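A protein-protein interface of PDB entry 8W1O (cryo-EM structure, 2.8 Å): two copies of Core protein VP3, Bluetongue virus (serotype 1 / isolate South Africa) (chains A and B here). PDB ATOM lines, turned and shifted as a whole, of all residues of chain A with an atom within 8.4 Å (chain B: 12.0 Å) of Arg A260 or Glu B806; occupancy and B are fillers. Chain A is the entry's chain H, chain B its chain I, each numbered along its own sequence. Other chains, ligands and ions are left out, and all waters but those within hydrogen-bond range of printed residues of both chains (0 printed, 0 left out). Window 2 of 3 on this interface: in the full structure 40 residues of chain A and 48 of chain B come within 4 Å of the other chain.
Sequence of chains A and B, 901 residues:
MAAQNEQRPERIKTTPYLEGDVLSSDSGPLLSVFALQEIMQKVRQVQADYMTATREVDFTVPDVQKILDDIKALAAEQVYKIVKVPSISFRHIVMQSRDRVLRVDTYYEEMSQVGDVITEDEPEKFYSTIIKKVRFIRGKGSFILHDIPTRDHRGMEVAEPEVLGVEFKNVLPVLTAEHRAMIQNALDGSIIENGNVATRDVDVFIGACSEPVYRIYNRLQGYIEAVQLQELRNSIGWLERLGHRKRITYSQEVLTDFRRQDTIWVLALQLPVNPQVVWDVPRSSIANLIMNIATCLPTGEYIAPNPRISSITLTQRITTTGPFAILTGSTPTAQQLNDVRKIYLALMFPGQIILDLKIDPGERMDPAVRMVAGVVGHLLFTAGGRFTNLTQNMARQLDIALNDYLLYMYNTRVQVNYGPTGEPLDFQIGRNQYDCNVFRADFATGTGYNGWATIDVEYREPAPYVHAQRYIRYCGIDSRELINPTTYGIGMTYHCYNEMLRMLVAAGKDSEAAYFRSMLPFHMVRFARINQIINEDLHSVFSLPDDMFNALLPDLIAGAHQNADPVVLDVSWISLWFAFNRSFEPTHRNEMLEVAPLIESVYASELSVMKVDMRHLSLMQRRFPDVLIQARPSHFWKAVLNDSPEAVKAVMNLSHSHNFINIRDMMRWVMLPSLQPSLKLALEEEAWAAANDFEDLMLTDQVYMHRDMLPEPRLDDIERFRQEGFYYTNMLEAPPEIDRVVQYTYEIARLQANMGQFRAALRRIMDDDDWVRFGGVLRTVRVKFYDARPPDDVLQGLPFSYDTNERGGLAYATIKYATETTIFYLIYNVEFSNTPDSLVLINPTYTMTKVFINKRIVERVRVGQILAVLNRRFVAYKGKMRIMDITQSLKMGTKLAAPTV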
ATOM      1  N   ASP A 201      17.094 -15.181  18.026  1.00  0.00           N
ATOM      2  CA  ASP A 201      16.273 -15.154  19.226  1.00  0.00           C
ATOM      3  C   ASP A 201      16.777 -16.131  20.279  1.00  0.00           C
ATOM      4  O   ASP A 201      16.768 -15.802  21.466  1.00  0.00           O
ATOM      5  CB  ASP A 201      14.815 -15.484  18.852  1.00  0.00           C
ATOM      6  CG  ASP A 201      13.824 -15.344  20.012  1.00  0.00           C
ATOM      7  OD1 ASP A 201      14.207 -15.196  21.189  1.00  0.00           O
ATOM      8  OD2 ASP A 201      12.609 -15.334  19.721  1.00  0.00           O
ATOM      9  N   GLU A 253     -11.649   0.618  29.147  1.00  0.00           N
ATOM     10  CA  GLU A 253     -10.389   0.112  28.626  1.00  0.00           C
ATOM     11  C   GLU A 253     -10.554  -1.315  28.117  1.00  0.00           C
ATOM     12  O   GLU A 253     -11.229  -2.136  28.742  1.00  0.00           O
ATOM     13  CB  GLU A 253      -9.320   0.163  29.718  1.00  0.00           C
ATOM     14  CG  GLU A 253      -7.908  -0.049  29.233  1.00  0.00           C
ATOM     15  CD  GLU A 253      -6.881   0.219  30.315  1.00  0.00           C
ATOM     16  OE1 GLU A 253      -6.885  -0.506  31.331  1.00  0.00           O
ATOM     17  OE2 GLU A 253      -6.073   1.157  30.150  1.00  0.00           O
ATOM     18  N   THR A 256      -5.842  -5.367  23.958  1.00  0.00           N
ATOM     19  CA  THR A 256      -5.436  -5.607  22.583  1.00  0.00           C
ATOM     20  C   THR A 256      -4.629  -6.901  22.485  1.00  0.00           C
ATOM     21  O   THR A 256      -4.362  -7.577  23.480  1.00  0.00           O
ATOM     22  CB  THR A 256      -4.633  -4.421  22.049  1.00  0.00           C
ATOM     23  OG1 THR A 256      -3.356  -4.377  22.696  1.00  0.00           O
ATOM     24  CG2 THR A 256      -5.368  -3.118  22.305  1.00  0.00           C
ATOM     25  N   ASP A 257      -4.234  -7.255  21.264  1.00  0.00           N
ATOM     26  CA  ASP A 257      -3.473  -8.469  21.004  1.00  0.00           C
ATOM     27  C   ASP A 257      -1.987  -8.211  20.804  1.00  0.00           C
ATOM     28  O   ASP A 257      -1.261  -9.130  20.415  1.00  0.00           O
ATOM     29  CB  ASP A 257      -4.032  -9.192  19.775  1.00  0.00           C
ATOM     30  CG  ASP A 257      -5.214 -10.079  20.107  1.00  0.00           C
ATOM     31  OD1 ASP A 257      -5.476 -10.301  21.306  1.00  0.00           O
ATOM     32  OD2 ASP A 257      -5.881 -10.556  19.165  1.00  0.00           O
ATOM     33  N   PHE A 258      -1.520  -6.991  21.049  1.00  0.00           N
ATOM     34  CA  PHE A 258      -0.124  -6.652  20.805  1.00  0.00           C
ATOM     35  C   PHE A 258       0.792  -7.374  21.786  1.00  0.00           C
ATOM     36  O   PHE A 258       0.520  -7.428  22.987  1.00  0.00           O
ATOM     37  CB  PHE A 258       0.068  -5.140  20.915  1.00  0.00           C
ATOM     38  CG  PHE A 258       1.498  -4.698  20.828  1.00  0.00           C
ATOM     39  CD1 PHE A 258       2.201  -4.801  19.642  1.00  0.00           C
ATOM     40  CD2 PHE A 258       2.138  -4.173  21.936  1.00  0.00           C
ATOM     41  CE1 PHE A 258       3.515  -4.390  19.563  1.00  0.00           C
ATOM     42  CE2 PHE A 258       3.454  -3.762  21.864  1.00  0.00           C
ATOM     43  CZ  PHE A 258       4.142  -3.871  20.677  1.00  0.00           C
ATOM     44  N   ARG A 259       1.881  -7.933  21.263  1.00  0.00           N
ATOM     45  CA  ARG A 259       2.905  -8.578  22.073  1.00  0.00           C
ATOM     46  C   ARG A 259       4.267  -8.053  21.654  1.00  0.00           C
ATOM     47  O   ARG A 259       4.561  -7.966  20.458  1.00  0.00           O
ATOM     48  CB  ARG A 259       2.858 -10.101  21.931  1.00  0.00           C
ATOM     49  CG  ARG A 259       3.389 -10.839  23.145  1.00  0.00           C
ATOM     50  CD  ARG A 259       4.151 -12.086  22.754  1.00  0.00           C
ATOM     51  NE  ARG A 259       3.298 -13.032  22.047  1.00  0.00           N
ATOM     52  CZ  ARG A 259       3.747 -14.013  21.279  1.00  0.00           C
ATOM     53  NH1 ARG A 259       5.043 -14.215  21.103  1.00  0.00           N
ATOM     54  NH2 ARG A 259       2.876 -14.810  20.669  1.00  0.00           N
ATOM     55  N   ARG A 260       5.091  -7.702  22.637  1.00  0.00           N
ATOM     56  CA  ARG A 260       6.419  -7.185  22.353  1.00  0.00           C
ATOM     57  C   ARG A 260       7.311  -8.271  21.764  1.00  0.00           C
ATOM     58  O   ARG A 260       7.124  -9.464  22.013  1.00  0.00           O
ATOM     59  CB  ARG A 260       7.054  -6.618  23.622  1.00  0.00           C
ATOM     60  CG  ARG A 260       6.411  -5.340  24.121  1.00  0.00           C
ATOM     61  CD  ARG A 260       6.916  -4.986  25.505  1.00  0.00           C
ATOM     62  NE  ARG A 260       8.372  -4.936  25.552  1.00  0.00           N
ATOM     63  CZ  ARG A 260       9.069  -4.032  26.225  1.00  0.00           C
ATOM     64  NH1 ARG A 260       8.473  -3.080  26.924  1.00  0.00           N
ATOM     65  NH2 ARG A 260      10.397  -4.087  26.200  1.00  0.00           N
ATOM     66  N   GLN A 261       8.293  -7.839  20.970  1.00  0.00           N
ATOM     67  CA  GLN A 261       9.190  -8.769  20.293  1.00  0.00           C
ATOM     68  C   GLN A 261      10.066  -9.557  21.259  1.00  0.00           C
ATOM     69  O   GLN A 261      10.551 -10.632  20.894  1.00  0.00           O
ATOM     70  CB  GLN A 261      10.079  -8.010  19.306  1.00  0.00           C
ATOM     71  CG  GLN A 261       9.341  -7.365  18.141  1.00  0.00           C
ATOM     72  CD  GLN A 261       8.646  -8.374  17.253  1.00  0.00           C
ATOM     73  OE1 GLN A 261       7.420  -8.467  17.238  1.00  0.00           O
ATOM     74  NE2 GLN A 261       9.430  -9.131  16.497  1.00  0.00           N
ATOM     75  N   ASP A 262      10.283  -9.057  22.473  1.00  0.00           N
ATOM     76  CA  ASP A 262      11.211  -9.667  23.421  1.00  0.00           C
ATOM     77  C   ASP A 262      10.518 -10.150  24.694  1.00  0.00           C
ATOM     78  O   ASP A 262      11.032  -9.977  25.800  1.00  0.00           O
ATOM     79  CB  ASP A 262      12.334  -8.693  23.768  1.00  0.00           C
ATOM     80  CG  ASP A 262      11.821  -7.389  24.345  1.00  0.00           C
ATOM     81  OD1 ASP A 262      10.592  -7.169  24.333  1.00  0.00           O
ATOM     82  OD2 ASP A 262      12.648  -6.582  24.815  1.00  0.00           O
ATOM     83  N   THR A 263       9.351 -10.775  24.558  1.00  0.00           N
ATOM     84  CA  THR A 263       8.593 -11.229  25.714  1.00  0.00           C
ATOM     85  C   THR A 263       7.977 -12.590  25.424  1.00  0.00           C
ATOM     86  O   THR A 263       7.450 -12.820  24.332  1.00  0.00           O
ATOM     87  CB  THR A 263       7.503 -10.212  26.085  1.00  0.00           C
ATOM     88  OG1 THR A 263       8.112  -8.949  26.371  1.00  0.00           O
ATOM     89  CG2 THR A 263       6.719 -10.665  27.306  1.00  0.00           C
ATOM     90  N   ILE A 264       8.051 -13.489  26.404  1.00  0.00           N
ATOM     91  CA  ILE A 264       7.436 -14.810  26.330  1.00  0.00           C
ATOM     92  C   ILE A 264       6.407 -14.925  27.445  1.00  0.00           C
ATOM     93  O   ILE A 264       6.724 -14.682  28.615  1.00  0.00           O
ATOM     94  CB  ILE A 264       8.479 -15.937  26.444  1.00  0.00           C
ATOM     95  CG1 ILE A 264       9.658 -15.681  25.508  1.00  0.00           C
ATOM     96  CG2 ILE A 264       7.842 -17.277  26.139  1.00  0.00           C
ATOM     97  CD1 ILE A 264       9.277 -15.691  24.050  1.00  0.00           C
ATOM     98  N   TRP A 265       5.185 -15.300  27.084  1.00  0.00           N
ATOM     99  CA  TRP A 265       4.130 -15.521  28.061  1.00  0.00           C
ATOM    100  C   TRP A 265       4.152 -16.960  28.562  1.00  0.00           C
ATOM    101  O   TRP A 265       4.588 -17.881  27.869  1.00  0.00           O
ATOM    102  CB  TRP A 265       2.755 -15.219  27.468  1.00  0.00           C
ATOM    103  CG  TRP A 265       2.511 -13.785  27.136  1.00  0.00           C
ATOM    104  CD1 TRP A 265       3.139 -12.699  27.666  1.00  0.00           C
ATOM    105  CD2 TRP A 265       1.542 -13.279  26.215  1.00  0.00           C
ATOM    106  NE1 TRP A 265       2.632 -11.546  27.119  1.00  0.00           N
ATOM    107  CE2 TRP A 265       1.647 -11.877  26.225  1.00  0.00           C
ATOM    108  CE3 TRP A 265       0.598 -13.879  25.376  1.00  0.00           C
ATOM    109  CZ2 TRP A 265       0.842 -11.063  25.432  1.00  0.00           C
ATOM    110  CZ3 TRP A 265      -0.196 -13.070  24.588  1.00  0.00           C
ATOM    111  CH2 TRP A 265      -0.068 -11.678  24.619  1.00  0.00           C
ATOM    112  N   LYS A 880      18.468 -10.773  26.186  1.00  0.00           N
ATOM    113  CA  LYS A 880      17.535  -9.685  25.927  1.00  0.00           C
ATOM    114  C   LYS A 880      16.089 -10.090  26.173  1.00  0.00           C
ATOM    115  O   LYS A 880      15.222  -9.215  26.261  1.00  0.00           O
ATOM    116  CB  LYS A 880      17.687  -9.191  24.488  1.00  0.00           C
ATOM    117  CG  LYS A 880      16.948 -10.041  23.470  1.00  0.00           C
ATOM    118  CD  LYS A 880      17.222  -9.593  22.049  1.00  0.00           C
ATOM    119  CE  LYS A 880      16.285 -10.282  21.074  1.00  0.00           C
ATOM    120  NZ  LYS A 880      16.621  -9.971  19.660  1.00  0.00           N
ATOM    121  N   MET A 881      15.809 -11.385  26.286  1.00  0.00           N
ATOM    122  CA  MET A 881      14.435 -11.847  26.357  1.00  0.00           C
ATOM    123  C   MET A 881      13.916 -11.788  27.791  1.00  0.00           C
ATOM    124  O   MET A 881      14.679 -11.791  28.761  1.00  0.00           O
ATOM    125  CB  MET A 881      14.320 -13.271  25.811  1.00  0.00           C
ATOM    126  CG  MET A 881      14.630 -13.383  24.330  1.00  0.00           C
ATOM    127  SD  MET A 881      13.536 -12.419  23.271  1.00  0.00           S
ATOM    128  CE  MET A 881      12.000 -13.315  23.454  1.00  0.00           C
ATOM    129  N   ARG A 882      12.593 -11.734  27.911  1.00  0.00           N
ATOM    130  CA  ARG A 882      11.911 -11.572  29.188  1.00  0.00           C
ATOM    131  C   ARG A 882      10.853 -12.655  29.329  1.00  0.00           C
ATOM    132  O   ARG A 882      10.048 -12.860  28.416  1.00  0.00           O
ATOM    133  CB  ARG A 882      11.283 -10.177  29.273  1.00  0.00           C
ATOM    134  CG  ARG A 882      12.317  -9.065  29.212  1.00  0.00           C
ATOM    135  CD  ARG A 882      11.725  -7.720  28.821  1.00  0.00           C
ATOM    136  NE  ARG A 882      10.503  -7.366  29.532  1.00  0.00           N
ATOM    137  CZ  ARG A 882       9.395  -6.963  28.927  1.00  0.00           C
ATOM    138  NH1 ARG A 882       9.303  -6.933  27.608  1.00  0.00           N
ATOM    139  NH2 ARG A 882       8.356  -6.577  29.659  1.00  0.00           N
ATOM    140  N   MET A 884       7.688 -13.953  31.604  1.00  0.00           N
ATOM    141  CA  MET A 884       6.699 -13.520  32.583  1.00  0.00           C
ATOM    142  C   MET A 884       5.545 -14.506  32.673  1.00  0.00           C
ATOM    143  O   MET A 884       5.168 -15.136  31.681  1.00  0.00           O
ATOM    144  CB  MET A 884       6.141 -12.125  32.261  1.00  0.00           C
ATOM    145  CG  MET A 884       7.183 -11.116  31.830  1.00  0.00           C
ATOM    146  SD  MET A 884       6.592  -9.424  31.980  1.00  0.00           S
ATOM    147  CE  MET A 884       8.153  -8.570  32.147  1.00  0.00           C
ATOM    148  N   ASN B 754      -6.906  -2.771  17.738  1.00  0.00           N
ATOM    149  CA  ASN B 754      -6.379  -4.106  17.997  1.00  0.00           C
ATOM    150  C   ASN B 754      -5.396  -4.525  16.914  1.00  0.00           C
ATOM    151  O   ASN B 754      -4.366  -5.142  17.207  1.00  0.00           O
ATOM    152  CB  ASN B 754      -7.520  -5.116  18.107  1.00  0.00           C
ATOM    153  CG  ASN B 754      -7.022  -6.535  18.279  1.00  0.00           C
ATOM    154  OD1 ASN B 754      -6.246  -6.823  19.187  1.00  0.00           O
ATOM    155  ND2 ASN B 754      -7.461  -7.428  17.406  1.00  0.00           N
ATOM    156  N   ARG B 759      -4.591   5.210  13.684  1.00  0.00           N
ATOM    157  CA  ARG B 759      -3.974   6.454  13.240  1.00  0.00           C
ATOM    158  C   ARG B 759      -3.661   6.419  11.752  1.00  0.00           C
ATOM    159  O   ARG B 759      -3.842   7.422  11.051  1.00  0.00           O
ATOM    160  CB  ARG B 759      -2.702   6.720  14.042  1.00  0.00           C
ATOM    161  CG  ARG B 759      -2.820   6.402  15.518  1.00  0.00           C
ATOM    162  CD  ARG B 759      -1.628   6.934  16.285  1.00  0.00           C
ATOM    163  NE  ARG B 759      -1.948   7.167  17.688  1.00  0.00           N
ATOM    164  CZ  ARG B 759      -1.371   6.536  18.701  1.00  0.00           C
ATOM    165  NH1 ARG B 759      -0.443   5.614  18.502  1.00  0.00           N
ATOM    166  NH2 ARG B 759      -1.737   6.833  19.943  1.00  0.00           N
ATOM    167  N   TYR B 802      -7.240   8.950  22.224  1.00  0.00           N
ATOM    168  CA  TYR B 802      -6.760   7.582  22.048  1.00  0.00           C
ATOM    169  C   TYR B 802      -5.516   7.401  22.905  1.00  0.00           C
ATOM    170  O   TYR B 802      -4.494   8.050  22.662  1.00  0.00           O
ATOM    171  CB  TYR B 802      -6.469   7.298  20.575  1.00  0.00           C
ATOM    172  CG  TYR B 802      -5.868   5.943  20.292  1.00  0.00           C
ATOM    173  CD1 TYR B 802      -6.349   4.803  20.918  1.00  0.00           C
ATOM    174  CD2 TYR B 802      -4.832   5.804  19.382  1.00  0.00           C
ATOM    175  CE1 TYR B 802      -5.803   3.563  20.655  1.00  0.00           C
ATOM    176  CE2 TYR B 802      -4.281   4.571  19.113  1.00  0.00           C
ATOM    177  CZ  TYR B 802      -4.770   3.454  19.750  1.00  0.00           C
ATOM    178  OH  TYR B 802      -4.223   2.223  19.482  1.00  0.00           O
ATOM    179  N   ASP B 803      -5.598   6.524  23.903  1.00  0.00           N
ATOM    180  CA  ASP B 803      -4.510   6.292  24.840  1.00  0.00           C
ATOM    181  C   ASP B 803      -4.151   4.813  24.884  1.00  0.00           C
ATOM    182  O   ASP B 803      -5.005   3.942  24.697  1.00  0.00           O
ATOM    183  CB  ASP B 803      -4.874   6.770  26.247  1.00  0.00           C
ATOM    184  CG  ASP B 803      -5.159   8.256  26.303  1.00  0.00           C
ATOM    185  OD1 ASP B 803      -4.297   9.044  25.863  1.00  0.00           O
ATOM    186  OD2 ASP B 803      -6.246   8.637  26.787  1.00  0.00           O
ATOM    187  N   THR B 804      -2.873   4.541  25.136  1.00  0.00           N
ATOM    188  CA  THR B 804      -2.354   3.186  25.232  1.00  0.00           C
ATOM    189  C   THR B 804      -1.567   3.041  26.527  1.00  0.00           C
ATOM    190  O   THR B 804      -0.750   3.897  26.874  1.00  0.00           O
ATOM    191  CB  THR B 804      -1.459   2.838  24.031  1.00  0.00           C
ATOM    192  OG1 THR B 804      -2.194   3.028  22.817  1.00  0.00           O
ATOM    193  CG2 THR B 804      -0.990   1.395  24.105  1.00  0.00           C
ATOM    194  N   ASN B 805      -1.822   1.946  27.240  1.00  0.00           N
ATOM    195  CA  ASN B 805      -1.182   1.698  28.521  1.00  0.00           C
ATOM    196  C   ASN B 805      -0.858   0.216  28.635  1.00  0.00           C
ATOM    197  O   ASN B 805      -1.637  -0.643  28.215  1.00  0.00           O
ATOM    198  CB  ASN B 805      -2.072   2.161  29.681  1.00  0.00           C
ATOM    199  CG  ASN B 805      -1.612   1.629  31.020  1.00  0.00           C
ATOM    200  OD1 ASN B 805      -0.472   1.845  31.429  1.00  0.00           O
ATOM    201  ND2 ASN B 805      -2.501   0.928  31.712  1.00  0.00           N
ATOM    202  N   GLU B 806       0.305  -0.076  29.214  1.00  0.00           N
ATOM    203  CA  GLU B 806       0.815  -1.437  29.318  1.00  0.00           C
ATOM    204  C   GLU B 806       1.034  -1.796  30.779  1.00  0.00           C
ATOM    205  O   GLU B 806       1.610  -1.006  31.534  1.00  0.00           O
ATOM    206  CB  GLU B 806       2.124  -1.589  28.540  1.00  0.00           C
ATOM    207  CG  GLU B 806       2.677  -3.003  28.521  1.00  0.00           C
ATOM    208  CD  GLU B 806       4.180  -3.032  28.328  1.00  0.00           C
ATOM    209  OE1 GLU B 806       4.645  -2.716  27.213  1.00  0.00           O
ATOM    210  OE2 GLU B 806       4.897  -3.367  29.294  1.00  0.00           O
ATOM    211  N   ARG B 807       0.580  -2.984  31.174  1.00  0.00           N
ATOM    212  CA  ARG B 807       0.825  -3.477  32.522  1.00  0.00           C
ATOM    213  C   ARG B 807       0.756  -4.998  32.526  1.00  0.00           C
ATOM    214  O   ARG B 807      -0.084  -5.591  31.845  1.00  0.00           O
ATOM    215  CB  ARG B 807      -0.171  -2.884  33.526  1.00  0.00           C
ATOM    216  CG  ARG B 807      -1.612  -3.307  33.336  1.00  0.00           C
ATOM    217  CD  ARG B 807      -2.519  -2.572  34.302  1.00  0.00           C
ATOM    218  NE  ARG B 807      -3.902  -3.018  34.199  1.00  0.00           N
ATOM    219  CZ  ARG B 807      -4.787  -2.519  33.348  1.00  0.00           C
ATOM    220  NH1 ARG B 807      -4.466  -1.557  32.500  1.00  0.00           N
ATOM    221  NH2 ARG B 807      -6.029  -2.998  33.350  1.00  0.00           N
ATOM    222  N   GLY B 808       1.657  -5.617  33.284  1.00  0.00           N
ATOM    223  CA  GLY B 808       1.690  -7.061  33.409  1.00  0.00           C
ATOM    224  C   GLY B 808       2.114  -7.779  32.145  1.00  0.00           C
ATOM    225  O   GLY B 808       1.897  -8.986  32.010  1.00  0.00           O
ATOM    226  N   GLY B 809       2.727  -7.053  31.216  1.00  0.00           N
ATOM    227  CA  GLY B 809       3.080  -7.612  29.929  1.00  0.00           C
ATOM    228  C   GLY B 809       1.971  -7.608  28.902  1.00  0.00           C
ATOM    229  O   GLY B 809       2.111  -8.264  27.864  1.00  0.00           O
ATOM    230  N   LEU B 810       0.879  -6.892  29.154  1.00  0.00           N
ATOM    231  CA  LEU B 810      -0.251  -6.811  28.243  1.00  0.00           C
ATOM    232  C   LEU B 810      -0.522  -5.354  27.897  1.00  0.00           C
ATOM    233  O   LEU B 810      -0.308  -4.457  28.716  1.00  0.00           O
ATOM    234  CB  LEU B 810      -1.507  -7.443  28.857  1.00  0.00           C
ATOM    235  CG  LEU B 810      -1.423  -8.907  29.295  1.00  0.00           C
ATOM    236  CD1 LEU B 810      -2.748  -9.366  29.884  1.00  0.00           C
ATOM    237  CD2 LEU B 810      -1.023  -9.795  28.140  1.00  0.00           C
ATOM    238  N   ALA B 811      -1.003  -5.122  26.679  1.00  0.00           N
ATOM    239  CA  ALA B 811      -1.249  -3.780  26.170  1.00  0.00           C
ATOM    240  C   ALA B 811      -2.744  -3.497  26.133  1.00  0.00           C
ATOM    241  O   ALA B 811      -3.544  -4.373  25.795  1.00  0.00           O
ATOM    242  CB  ALA B 811      -0.649  -3.603  24.773  1.00  0.00           C
ATOM    243  N   TYR B 812      -3.113  -2.264  26.476  1.00  0.00           N
ATOM    244  CA  TYR B 812      -4.505  -1.853  26.567  1.00  0.00           C
ATOM    245  C   TYR B 812      -4.724  -0.577  25.768  1.00  0.00           C
ATOM    246  O   TYR B 812      -3.788   0.184  25.515  1.00  0.00           O
ATOM    247  CB  TYR B 812      -4.926  -1.628  28.023  1.00  0.00           C
ATOM    248  CG  TYR B 812      -4.911  -2.875  28.874  1.00  0.00           C
ATOM    249  CD1 TYR B 812      -3.731  -3.348  29.432  1.00  0.00           C
ATOM    250  CD2 TYR B 812      -6.078  -3.582  29.121  1.00  0.00           C
ATOM    251  CE1 TYR B 812      -3.715  -4.488  30.206  1.00  0.00           C
ATOM    252  CE2 TYR B 812      -6.072  -4.722  29.894  1.00  0.00           C
ATOM    253  CZ  TYR B 812      -4.887  -5.170  30.434  1.00  0.00           C
ATOM    254  OH  TYR B 812      -4.880  -6.307  31.207  1.00  0.00           O
ATOM    255  N   ALA B 813      -5.975  -0.352  25.368  1.00  0.00           N
ATOM    256  CA  ALA B 813      -6.357   0.827  24.603  1.00  0.00           C
ATOM    257  C   ALA B 813      -7.642   1.419  25.162  1.00  0.00           C
ATOM    258  O   ALA B 813      -8.523   0.689  25.620  1.00  0.00           O
ATOM    259  CB  ALA B 813      -6.542   0.495  23.119  1.00  0.00           C
ATOM    260  N   THR B 814      -7.741   2.746  25.120  1.00  0.00           N
ATOM    261  CA  THR B 814      -8.933   3.470  25.541  1.00  0.00           C
ATOM    262  C   THR B 814      -9.271   4.515  24.490  1.00  0.00           C
ATOM    263  O   THR B 814      -8.427   5.351  24.151  1.00  0.00           O
ATOM    264  CB  THR B 814      -8.730   4.142  26.904  1.00  0.00           C
ATOM    265  OG1 THR B 814      -8.335   3.161  27.870  1.00  0.00           O
ATOM    266  CG2 THR B 814     -10.014   4.806  27.365  1.00  0.00           C
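Printed residues of chain B that touch a printed residue of chain A: Asn B754, Asn B805, Glu B806, Arg B807, Gly B809, Leu B810, Ala B811, Tyr B812, Ala B813 and Thr B814. Hydrophobic or aromatic side chains of chain B within 4 Å of the printed part of chain A: Leu B810, Ala B811, Tyr B812 and Ala B813. Of the 16 printed residues of chain A, 5 touch a printed residue of chain B. Printed residues of chain A that touch a printed residue of chain B: Glu A253, Thr A256, Asp A257, Arg A260 and Trp A265. Hydrophobic or aromatic side chains of chain A within 4 Å of the printed part of chain B: Trp A265. Along chain A the printed residues that touch a printed residue of chain B span positions 253 to 265. Among the printed residues, Asp or Glu carboxylates within 4 Å of a Lys or Arg side-chain nitrogen of the other chain: Glu A253 with Arg B807 and Arg A260 with Glu B806.
NE1 of Trp A265 sits at hydrogen-bond distance from O of Gly B809 (3.4 Å). The backbone NH of Asp A257 lies within hydrogen-bond range of the side-chain amide oxygen of Asn B754. NH1 of Arg B807 is in salt-bridge range of OE1 of Glu A253, 2.9 Å away. The side-chain hydroxyl of Thr A256 is in hydrogen-bond range of the backbone carbonyl oxygen of Ala B811 (3.1 Å). The guanidinium group (NH1) of Arg A260 lies within salt-bridge range of the side-chain carboxylate (OE1) of Glu B806 (3.9 Å).
No position is printed for both chains.
OD1 of Asp A262 is in salt-bridge range of NE of Arg A260, 3.4 Å away. O of Asp B803 sits at hydrogen-bond distance from N of Thr B814 (3.0 Å). O of Asn B805 lies within hydrogen-bond range of N of Tyr B812, 2.8 Å away. NH1 of Arg B807 lies close to ND2 of Asn B805, 3.3 Å away.
Among the printed residues, merely in contact across the chains: Glu A253 with Asn B805 (3.9 Å), Glu A253 with Tyr B812 (3.5 Å), Glu A253 with Ala B813 (3.6 Å), Glu A253 with Thr B814 (3.5 Å), Thr A256 with Asn B754 (3.7 Å), Thr A256 with Ala B813 (3.9 Å) and Trp A265 with Leu B810 (3.5 Å).
Arg A260 touches one residue of chain B. Glu B806 touches just one residue of chain A: Arg A260 (3.6 Å). No residue of chain B comes within 4 Å of Arg A259. No residue of chain B comes within 4 Å of Gln A261. No residue of chain B comes within 4 Å of Asp A262. No residue of chain B comes within 4 Å of Thr A263. Printed residues of chain B within 4 Å of Glu A253: Asn B805, Arg B807, Tyr B812, Ala B813 and Thr B814. Of the printed residues of chain A, Asn B754 touches Thr A256 (3.7 Å) and Asp A257 (2.9 Å). Of the printed residues of chain A, Thr B814 touches Glu A253 (3.5 Å). Of the printed residues of chain B, Trp A265 touches Gly B809 (3.4 Å) and Leu B810 (3.5 Å). The nearest residue of chain B that does not touch Arg A260 is Gly B809 (6.0 Å). The nearest printed residue of chain A that does not touch Leu B810 is Phe A258 (5.3 Å).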
